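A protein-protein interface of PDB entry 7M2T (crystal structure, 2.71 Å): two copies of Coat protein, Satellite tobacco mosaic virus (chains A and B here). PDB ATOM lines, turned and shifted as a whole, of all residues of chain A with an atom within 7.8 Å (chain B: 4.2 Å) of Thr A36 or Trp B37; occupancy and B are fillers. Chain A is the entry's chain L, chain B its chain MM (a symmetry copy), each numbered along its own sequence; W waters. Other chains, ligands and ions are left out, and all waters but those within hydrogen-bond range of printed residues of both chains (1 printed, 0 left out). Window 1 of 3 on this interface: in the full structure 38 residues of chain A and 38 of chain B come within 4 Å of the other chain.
The guanidinium group (NH2) of Arg B39 is in hydrogen-bond range of the backbone carbonyl oxygen (O) of Pro A33, at 2.9 Å.
The guanidinium group (NH2) of Arg B66 sits at hydrogen-bond distance from the backbone carbonyl oxygen (O) of Thr A34.
The backbone carbonyl oxygen of Pro A35 lies within hydrogen-bond range of the guanidinium group of Arg B66, at 2.9 Å.
The guanidinium group (NH1) of Arg B66 sits at hydrogen-bond distance from the side-chain hydroxyl (OG) of Ser A69 (3.0 Å).
The indole nitrogen (NE1) of Trp A37 sits close to the indole nitrogen (NE1) of Trp B37.
N of Thr A34 sits at hydrogen-bond distance from OD1 of Asn A32, 3.1 Å away.
O of Trp A37 is in hydrogen-bond range of N of Phe A158 (2.8 Å).
The backbone NH (N) of Phe B158 sits at hydrogen-bond distance from the backbone carbonyl oxygen (O) of Trp B37.
O of Cys B156 sits at hydrogen-bond distance from N of Arg B39, at 2.9 Å.
Trp B37 touches Pro A35.
Pro A35 touches Arg B39 (CD to NH2, 3.3 Å).
O of Thr A36 touches CZ2 of Trp B37, at 3.8 Å.
Trp A37 touches Thr B36 (CZ2 to O, 3.6 Å).
Phe A70 touches Arg B66.
Of the printed residues of chain B, Thr A36 touches Trp B37.
Trp B37 touches just these residues of chain A: Pro A35 (3.9 Å), Thr A36 (3.8 Å) and Trp A37 (3.4 Å).
Of the printed residues of chain B, Thr A34 touches Arg B66 (3.1 Å).
Printed residues of chain B within 4 Å of Pro A35: Trp B37 (3.9 Å), Arg B39 (3.3 Å) and Arg B66 (2.9 Å).
Printed residues of chain B within 4 Å of Pro A33: Arg B39.
Phe A65 touches none of the printed residues of chain B.
Cys B156 touches none of the printed residues of chain A.
The nearest residue of chain A that does not touch Trp B37 is Phe A70 (4.6 Å).
Thr A36 touches Trp B37, and with the chains exchanged Trp A37 touches Thr B36.
Trp B37 touches its own counterpart, Trp A37.
7 positions are printed for both chains.
Of the 10 pairs that touch across the chains among the printed residues, 3 have their exchanged pair printed and touching as well.
Water W1 lies within hydrogen-bond range of O of Asn A32 (2.6 Å) and NH2 of Arg B39 (2.6 Å).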
ATOM      1  N   ASN A  32      -3.641 -22.391 -12.958  1.00  0.00           N
ATOM      2  CA  ASN A  32      -2.657 -23.122 -12.177  1.00  0.00           C
ATOM      3  C   ASN A  32      -2.709 -22.634 -10.738  1.00  0.00           C
ATOM      4  O   ASN A  32      -2.298 -21.504 -10.450  1.00  0.00           O
ATOM      5  CB  ASN A  32      -1.253 -22.945 -12.749  1.00  0.00           C
ATOM      6  CG  ASN A  32      -0.182 -23.585 -11.880  1.00  0.00           C
ATOM      7  OD1 ASN A  32      -0.450 -24.526 -11.127  1.00  0.00           O
ATOM      8  ND2 ASN A  32       1.037 -23.076 -11.981  1.00  0.00           N
ATOM      9  N   PRO A  33      -3.195 -23.457  -9.808  1.00  0.00           N
ATOM     10  CA  PRO A  33      -3.318 -23.000  -8.417  1.00  0.00           C
ATOM     11  C   PRO A  33      -1.995 -22.932  -7.675  1.00  0.00           C
ATOM     12  O   PRO A  33      -1.937 -22.307  -6.609  1.00  0.00           O
ATOM     13  CB  PRO A  33      -4.247 -24.047  -7.793  1.00  0.00           C
ATOM     14  CG  PRO A  33      -3.945 -25.294  -8.563  1.00  0.00           C
ATOM     15  CD  PRO A  33      -3.623 -24.857  -9.973  1.00  0.00           C
ATOM     16  N   THR A  34      -0.934 -23.545  -8.200  1.00  0.00           N
ATOM     17  CA  THR A  34       0.353 -23.642  -7.510  1.00  0.00           C
ATOM     18  C   THR A  34       1.479 -23.206  -8.444  1.00  0.00           C
ATOM     19  O   THR A  34       2.234 -24.041  -8.961  1.00  0.00           O
ATOM     20  CB  THR A  34       0.573 -25.064  -7.001  1.00  0.00           C
ATOM     21  OG1 THR A  34       0.254 -25.991  -8.046  1.00  0.00           O
ATOM     22  CG2 THR A  34      -0.323 -25.339  -5.805  1.00  0.00           C
ATOM     23  N   PRO A  35       1.634 -21.905  -8.665  1.00  0.00           N
ATOM     24  CA  PRO A  35       2.620 -21.411  -9.632  1.00  0.00           C
ATOM     25  C   PRO A  35       4.033 -21.387  -9.055  1.00  0.00           C
ATOM     26  O   PRO A  35       4.267 -21.698  -7.888  1.00  0.00           O
ATOM     27  CB  PRO A  35       2.122 -19.998  -9.935  1.00  0.00           C
ATOM     28  CG  PRO A  35       1.442 -19.582  -8.685  1.00  0.00           C
ATOM     29  CD  PRO A  35       0.800 -20.818  -8.125  1.00  0.00           C
ATOM     30  N   THR A  36       4.978 -21.004  -9.913  1.00  0.00           N
ATOM     31  CA  THR A  36       6.371 -20.805  -9.544  1.00  0.00           C
ATOM     32  C   THR A  36       6.571 -19.409  -8.950  1.00  0.00           C
ATOM     33  O   THR A  36       5.709 -18.531  -9.049  1.00  0.00           O
ATOM     34  CB  THR A  36       7.277 -20.997 -10.761  1.00  0.00           C
ATOM     35  OG1 THR A  36       6.920 -20.050 -11.774  1.00  0.00           O
ATOM     36  CG2 THR A  36       7.112 -22.386 -11.330  1.00  0.00           C
ATOM     37  N   TRP A  37       7.731 -19.198  -8.335  1.00  0.00           N
ATOM     38  CA  TRP A  37       7.994 -17.942  -7.640  1.00  0.00           C
ATOM     39  C   TRP A  37       9.483 -17.639  -7.693  1.00  0.00           C
ATOM     40  O   TRP A  37      10.295 -18.421  -7.190  1.00  0.00           O
ATOM     41  CB  TRP A  37       7.510 -18.018  -6.190  1.00  0.00           C
ATOM     42  CG  TRP A  37       7.039 -16.716  -5.623  1.00  0.00           C
ATOM     43  CD1 TRP A  37       7.066 -15.494  -6.232  1.00  0.00           C
ATOM     44  CD2 TRP A  37       6.456 -16.506  -4.330  1.00  0.00           C
ATOM     45  NE1 TRP A  37       6.542 -14.536  -5.396  1.00  0.00           N
ATOM     46  CE2 TRP A  37       6.160 -15.133  -4.224  1.00  0.00           C
ATOM     47  CE3 TRP A  37       6.158 -17.347  -3.253  1.00  0.00           C
ATOM     48  CZ2 TRP A  37       5.580 -14.582  -3.083  1.00  0.00           C
ATOM     49  CZ3 TRP A  37       5.584 -16.797  -2.120  1.00  0.00           C
ATOM     50  CH2 TRP A  37       5.301 -15.428  -2.045  1.00  0.00           C
ATOM     51  N   VAL A  38       9.837 -16.512  -8.300  1.00  0.00           N
ATOM     52  CA  VAL A  38      11.211 -16.023  -8.298  1.00  0.00           C
ATOM     53  C   VAL A  38      11.412 -15.206  -7.031  1.00  0.00           C
ATOM     54  O   VAL A  38      10.674 -14.248  -6.779  1.00  0.00           O
ATOM     55  CB  VAL A  38      11.508 -15.185  -9.548  1.00  0.00           C
ATOM     56  CG1 VAL A  38      12.843 -14.491  -9.403  1.00  0.00           C
ATOM     57  CG2 VAL A  38      11.495 -16.067 -10.784  1.00  0.00           C
ATOM     58  N   ARG A  39      12.404 -15.584  -6.232  1.00  0.00           N
ATOM     59  CA  ARG A  39      12.543 -15.043  -4.890  1.00  0.00           C
ATOM     60  C   ARG A  39      14.000 -14.718  -4.599  1.00  0.00           C
ATOM     61  O   ARG A  39      14.914 -15.192  -5.276  1.00  0.00           O
ATOM     62  CB  ARG A  39      12.012 -16.030  -3.839  1.00  0.00           C
ATOM     63  CG  ARG A  39      10.522 -16.343  -3.968  1.00  0.00           C
ATOM     64  CD  ARG A  39       9.683 -15.179  -3.478  1.00  0.00           C
ATOM     65  NE  ARG A  39      10.047 -14.831  -2.111  1.00  0.00           N
ATOM     66  CZ  ARG A  39       9.562 -15.438  -1.037  1.00  0.00           C
ATOM     67  NH1 ARG A  39       8.654 -16.393  -1.135  1.00  0.00           N
ATOM     68  NH2 ARG A  39      10.004 -15.082   0.165  1.00  0.00           N
ATOM     69  N   PHE A  65       9.280 -17.961   4.855  1.00  0.00           N
ATOM     70  CA  PHE A  65       9.493 -17.377   3.536  1.00  0.00           C
ATOM     71  C   PHE A  65       8.293 -17.561   2.617  1.00  0.00           C
ATOM     72  O   PHE A  65       8.386 -17.240   1.426  1.00  0.00           O
ATOM     73  CB  PHE A  65      10.736 -17.980   2.874  1.00  0.00           C
ATOM     74  CG  PHE A  65      11.970 -17.916   3.718  1.00  0.00           C
ATOM     75  CD1 PHE A  65      12.341 -16.735   4.337  1.00  0.00           C
ATOM     76  CD2 PHE A  65      12.761 -19.041   3.893  1.00  0.00           C
ATOM     77  CE1 PHE A  65      13.486 -16.678   5.114  1.00  0.00           C
ATOM     78  CE2 PHE A  65      13.901 -18.993   4.667  1.00  0.00           C
ATOM     79  CZ  PHE A  65      14.266 -17.810   5.279  1.00  0.00           C
ATOM     80  N   ARG A  66       7.175 -18.071   3.142  1.00  0.00           N
ATOM     81  CA  ARG A  66       6.011 -18.464   2.342  1.00  0.00           C
ATOM     82  C   ARG A  66       6.364 -19.536   1.314  1.00  0.00           C
ATOM     83  O   ARG A  66       5.755 -19.601   0.244  1.00  0.00           O
ATOM     84  CB  ARG A  66       5.368 -17.270   1.628  1.00  0.00           C
ATOM     85  CG  ARG A  66       5.206 -16.000   2.436  1.00  0.00           C
ATOM     86  CD  ARG A  66       4.277 -15.069   1.679  1.00  0.00           C
ATOM     87  NE  ARG A  66       4.301 -13.691   2.157  1.00  0.00           N
ATOM     88  CZ  ARG A  66       3.530 -13.214   3.127  1.00  0.00           C
ATOM     89  NH1 ARG A  66       2.693 -13.993   3.792  1.00  0.00           N
ATOM     90  NH2 ARG A  66       3.594 -11.920   3.427  1.00  0.00           N
ATOM     91  N   THR A  67       7.348 -20.386   1.611  1.00  0.00           N
ATOM     92  CA  THR A  67       7.832 -21.357   0.635  1.00  0.00           C
ATOM     93  C   THR A  67       7.644 -22.804   1.070  1.00  0.00           C
ATOM     94  O   THR A  67       8.109 -23.710   0.367  1.00  0.00           O
ATOM     95  CB  THR A  67       9.313 -21.114   0.320  1.00  0.00           C
ATOM     96  OG1 THR A  67      10.088 -21.238   1.519  1.00  0.00           O
ATOM     97  CG2 THR A  67       9.514 -19.732  -0.279  1.00  0.00           C
ATOM     98  N   SER A  69       5.363 -24.841   0.803  1.00  0.00           N
ATOM     99  CA  SER A  69       4.618 -25.708  -0.101  1.00  0.00           C
ATOM    100  C   SER A  69       5.453 -26.209  -1.278  1.00  0.00           C
ATOM    101  O   SER A  69       4.993 -27.098  -2.002  1.00  0.00           O
ATOM    102  CB  SER A  69       3.369 -24.989  -0.624  1.00  0.00           C
ATOM    103  OG  SER A  69       3.699 -23.970  -1.556  1.00  0.00           O
ATOM    104  N   PHE A  70       6.649 -25.668  -1.492  1.00  0.00           N
ATOM    105  CA  PHE A  70       7.537 -26.157  -2.537  1.00  0.00           C
ATOM    106  C   PHE A  70       8.404 -27.287  -2.003  1.00  0.00           C
ATOM    107  O   PHE A  70       8.679 -27.374  -0.802  1.00  0.00           O
ATOM    108  CB  PHE A  70       8.442 -25.044  -3.068  1.00  0.00           C
ATOM    109  CG  PHE A  70       7.711 -23.923  -3.745  1.00  0.00           C
ATOM    110  CD1 PHE A  70       7.308 -24.036  -5.062  1.00  0.00           C
ATOM    111  CD2 PHE A  70       7.457 -22.740  -3.075  1.00  0.00           C
ATOM    112  CE1 PHE A  70       6.653 -22.999  -5.692  1.00  0.00           C
ATOM    113  CE2 PHE A  70       6.799 -21.700  -3.700  1.00  0.00           C
ATOM    114  CZ  PHE A  70       6.396 -21.829  -5.009  1.00  0.00           C
ATOM    115  N   CYS A 157      14.446 -19.751  -8.062  1.00  0.00           N
ATOM    116  CA  CYS A 157      13.113 -19.950  -8.616  1.00  0.00           C
ATOM    117  C   CYS A 157      12.519 -21.180  -7.950  1.00  0.00           C
ATOM    118  O   CYS A 157      12.981 -22.299  -8.191  1.00  0.00           O
ATOM    119  CB  CYS A 157      13.157 -20.137 -10.131  1.00  0.00           C
ATOM    120  SG  CYS A 157      14.177 -18.965 -11.042  1.00  0.00           S
ATOM    121  N   PHE A 158      11.510 -20.977  -7.106  1.00  0.00           N
ATOM    122  CA  PHE A 158      10.780 -22.097  -6.529  1.00  0.00           C
ATOM    123  C   PHE A 158       9.808 -22.677  -7.548  1.00  0.00           C
ATOM    124  O   PHE A 158       9.145 -21.944  -8.287  1.00  0.00           O
ATOM    125  CB  PHE A 158      10.028 -21.662  -5.272  1.00  0.00           C
ATOM    126  CG  PHE A 158      10.929 -21.340  -4.120  1.00  0.00           C
ATOM    127  CD1 PHE A 158      11.346 -22.335  -3.248  1.00  0.00           C
ATOM    128  CD2 PHE A 158      11.375 -20.042  -3.914  1.00  0.00           C
ATOM    129  CE1 PHE A 158      12.186 -22.042  -2.186  1.00  0.00           C
ATOM    130  CE2 PHE A 158      12.214 -19.741  -2.853  1.00  0.00           C
ATOM    131  CZ  PHE A 158      12.621 -20.742  -1.988  1.00  0.00           C
ATOM    132  N   ASN A 159       9.735 -24.001  -7.590  1.00  0.00           N
ATOM    133  CA  ASN A 159       8.843 -24.676  -8.520  1.00  0.00           C
ATOM    134  C   ASN A 159       8.520 -26.071  -8.010  1.00  0.00           C
ATOM    135  O   ASN A 159       7.499 -26.661  -8.365  1.00  0.00           O
ATOM    136  CB  ASN A 159       9.467 -24.748  -9.914  1.00  0.00           C
ATOM    137  CG  ASN A 159      10.626 -25.721  -9.986  1.00  0.00           C
ATOM    138  OD1 ASN A 159      10.463 -26.861 -10.417  1.00  0.00           O
ATOM    139  ND2 ASN A 159      11.806 -25.273  -9.573  1.00  0.00           N
ATOM    140  OXT ASN A 159       9.277 -26.629  -7.219  1.00  0.00           O
ATOM    141  N   THR B  36       4.762  -9.631  -1.146  1.00  0.00           N
ATOM    142  CA  THR B  36       3.421  -9.722  -1.700  1.00  0.00           C
ATOM    143  C   THR B  36       3.427 -10.665  -2.901  1.00  0.00           C
ATOM    144  O   THR B  36       4.464 -11.203  -3.299  1.00  0.00           O
ATOM    145  CB  THR B  36       2.901  -8.337  -2.088  1.00  0.00           C
ATOM    146  OG1 THR B  36       3.774  -7.743  -3.055  1.00  0.00           O
ATOM    147  CG2 THR B  36       2.826  -7.430  -0.878  1.00  0.00           C
ATOM    148  N   TRP B  37       2.252 -10.866  -3.496  1.00  0.00           N
ATOM    149  CA  TRP B  37       2.115 -11.831  -4.586  1.00  0.00           C
ATOM    150  C   TRP B  37       0.823 -11.545  -5.333  1.00  0.00           C
ATOM    151  O   TRP B  37      -0.259 -11.601  -4.740  1.00  0.00           O
ATOM    152  CB  TRP B  37       2.117 -13.260  -4.039  1.00  0.00           C
ATOM    153  CG  TRP B  37       2.639 -14.284  -4.989  1.00  0.00           C
ATOM    154  CD1 TRP B  37       3.095 -14.072  -6.254  1.00  0.00           C
ATOM    155  CD2 TRP B  37       2.765 -15.693  -4.746  1.00  0.00           C
ATOM    156  NE1 TRP B  37       3.494 -15.262  -6.819  1.00  0.00           N
ATOM    157  CE2 TRP B  37       3.303 -16.272  -5.913  1.00  0.00           C
ATOM    158  CE3 TRP B  37       2.476 -16.520  -3.655  1.00  0.00           C
ATOM    159  CZ2 TRP B  37       3.559 -17.638  -6.021  1.00  0.00           C
ATOM    160  CZ3 TRP B  37       2.730 -17.879  -3.765  1.00  0.00           C
ATOM    161  CH2 TRP B  37       3.267 -18.422  -4.940  1.00  0.00           C
ATOM    162  N   VAL B  38       0.932 -11.238  -6.623  1.00  0.00           N
ATOM    163  CA  VAL B  38      -0.231 -11.043  -7.482  1.00  0.00           C
ATOM    164  C   VAL B  38      -0.603 -12.387  -8.086  1.00  0.00           C
ATOM    165  O   VAL B  38       0.261 -13.108  -8.594  1.00  0.00           O
ATOM    166  CB  VAL B  38       0.056 -10.003  -8.576  1.00  0.00           C
ATOM    167  CG1 VAL B  38      -1.152  -9.844  -9.470  1.00  0.00           C
ATOM    168  CG2 VAL B  38       0.438  -8.672  -7.949  1.00  0.00           C
ATOM    169  N   ARG B  39      -1.884 -12.738  -8.018  1.00  0.00           N
ATOM    170  CA  ARG B  39      -2.293 -14.105  -8.300  1.00  0.00           C
ATOM    171  C   ARG B  39      -3.656 -14.118  -8.973  1.00  0.00           C
ATOM    172  O   ARG B  39      -4.451 -13.186  -8.832  1.00  0.00           O
ATOM    173  CB  ARG B  39      -2.340 -14.944  -7.015  1.00  0.00           C
ATOM    174  CG  ARG B  39      -1.006 -15.089  -6.292  1.00  0.00           C
ATOM    175  CD  ARG B  39      -0.136 -16.131  -6.961  1.00  0.00           C
ATOM    176  NE  ARG B  39      -0.873 -17.375  -7.135  1.00  0.00           N
ATOM    177  CZ  ARG B  39      -0.926 -18.340  -6.228  1.00  0.00           C
ATOM    178  NH1 ARG B  39      -0.253 -18.257  -5.094  1.00  0.00           N
ATOM    179  NH2 ARG B  39      -1.677 -19.412  -6.464  1.00  0.00           N
ATOM    180  N   ARG B  66      -0.800 -22.103  -2.175  1.00  0.00           N
ATOM    181  CA  ARG B  66       0.439 -21.581  -1.595  1.00  0.00           C
ATOM    182  C   ARG B  66       0.214 -20.255  -0.869  1.00  0.00           C
ATOM    183  O   ARG B  66       1.134 -19.442  -0.753  1.00  0.00           O
ATOM    184  CB  ARG B  66       1.538 -21.406  -2.650  1.00  0.00           C
ATOM    185  CG  ARG B  66       1.729 -22.546  -3.639  1.00  0.00           C
ATOM    186  CD  ARG B  66       3.007 -22.284  -4.430  1.00  0.00           C
ATOM    187  NE  ARG B  66       3.208 -23.171  -5.571  1.00  0.00           N
ATOM    188  CZ  ARG B  66       3.791 -24.361  -5.506  1.00  0.00           C
ATOM    189  NH1 ARG B  66       4.188 -24.877  -4.357  1.00  0.00           N
ATOM    190  NH2 ARG B  66       3.989 -25.045  -6.626  1.00  0.00           N
ATOM    191  N   CYS B 156      -6.075 -10.998  -7.622  1.00  0.00           N
ATOM    192  CA  CYS B 156      -5.923 -10.350  -6.329  1.00  0.00           C
ATOM    193  C   CYS B 156      -4.450 -10.213  -5.976  1.00  0.00           C
ATOM    194  O   CYS B 156      -3.584 -10.868  -6.562  1.00  0.00           O
ATOM    195  CB  CYS B 156      -6.662 -11.127  -5.239  1.00  0.00           C
ATOM    196  SG  CYS B 156      -6.216 -12.864  -5.170  1.00  0.00           S
ATOM    197  N   CYS B 157      -4.187  -9.349  -4.997  1.00  0.00           N
ATOM    198  CA  CYS B 157      -2.841  -9.075  -4.505  1.00  0.00           C
ATOM    199  C   CYS B 157      -2.772  -9.503  -3.045  1.00  0.00           C
ATOM    200  O   CYS B 157      -3.329  -8.831  -2.169  1.00  0.00           O
ATOM    201  CB  CYS B 157      -2.488  -7.594  -4.647  1.00  0.00           C
ATOM    202  SG  CYS B 157      -2.535  -6.938  -6.327  1.00  0.00           S
ATOM    203  N   PHE B 158      -2.095 -10.619  -2.784  1.00  0.00           N
ATOM    204  CA  PHE B 158      -1.896 -11.073  -1.417  1.00  0.00           C
ATOM    205  C   PHE B 158      -0.833 -10.220  -0.745  1.00  0.00           C
ATOM    206  O   PHE B 158       0.229  -9.969  -1.322  1.00  0.00           O
ATOM    207  CB  PHE B 158      -1.493 -12.548  -1.389  1.00  0.00           C
ATOM    208  CG  PHE B 158      -2.606 -13.477  -1.755  1.00  0.00           C
ATOM    209  CD1 PHE B 158      -3.478 -13.947  -0.786  1.00  0.00           C
ATOM    210  CD2 PHE B 158      -2.792 -13.872  -3.070  1.00  0.00           C
ATOM    211  CE1 PHE B 158      -4.511 -14.799  -1.120  1.00  0.00           C
ATOM    212  CE2 PHE B 158      -3.822 -14.725  -3.411  1.00  0.00           C
ATOM    213  CZ  PHE B 158      -4.683 -15.189  -2.437  1.00  0.00           C
HETATM  214  O   HOH W   1      -2.829 -19.572  -8.835  1.00  0.00           O
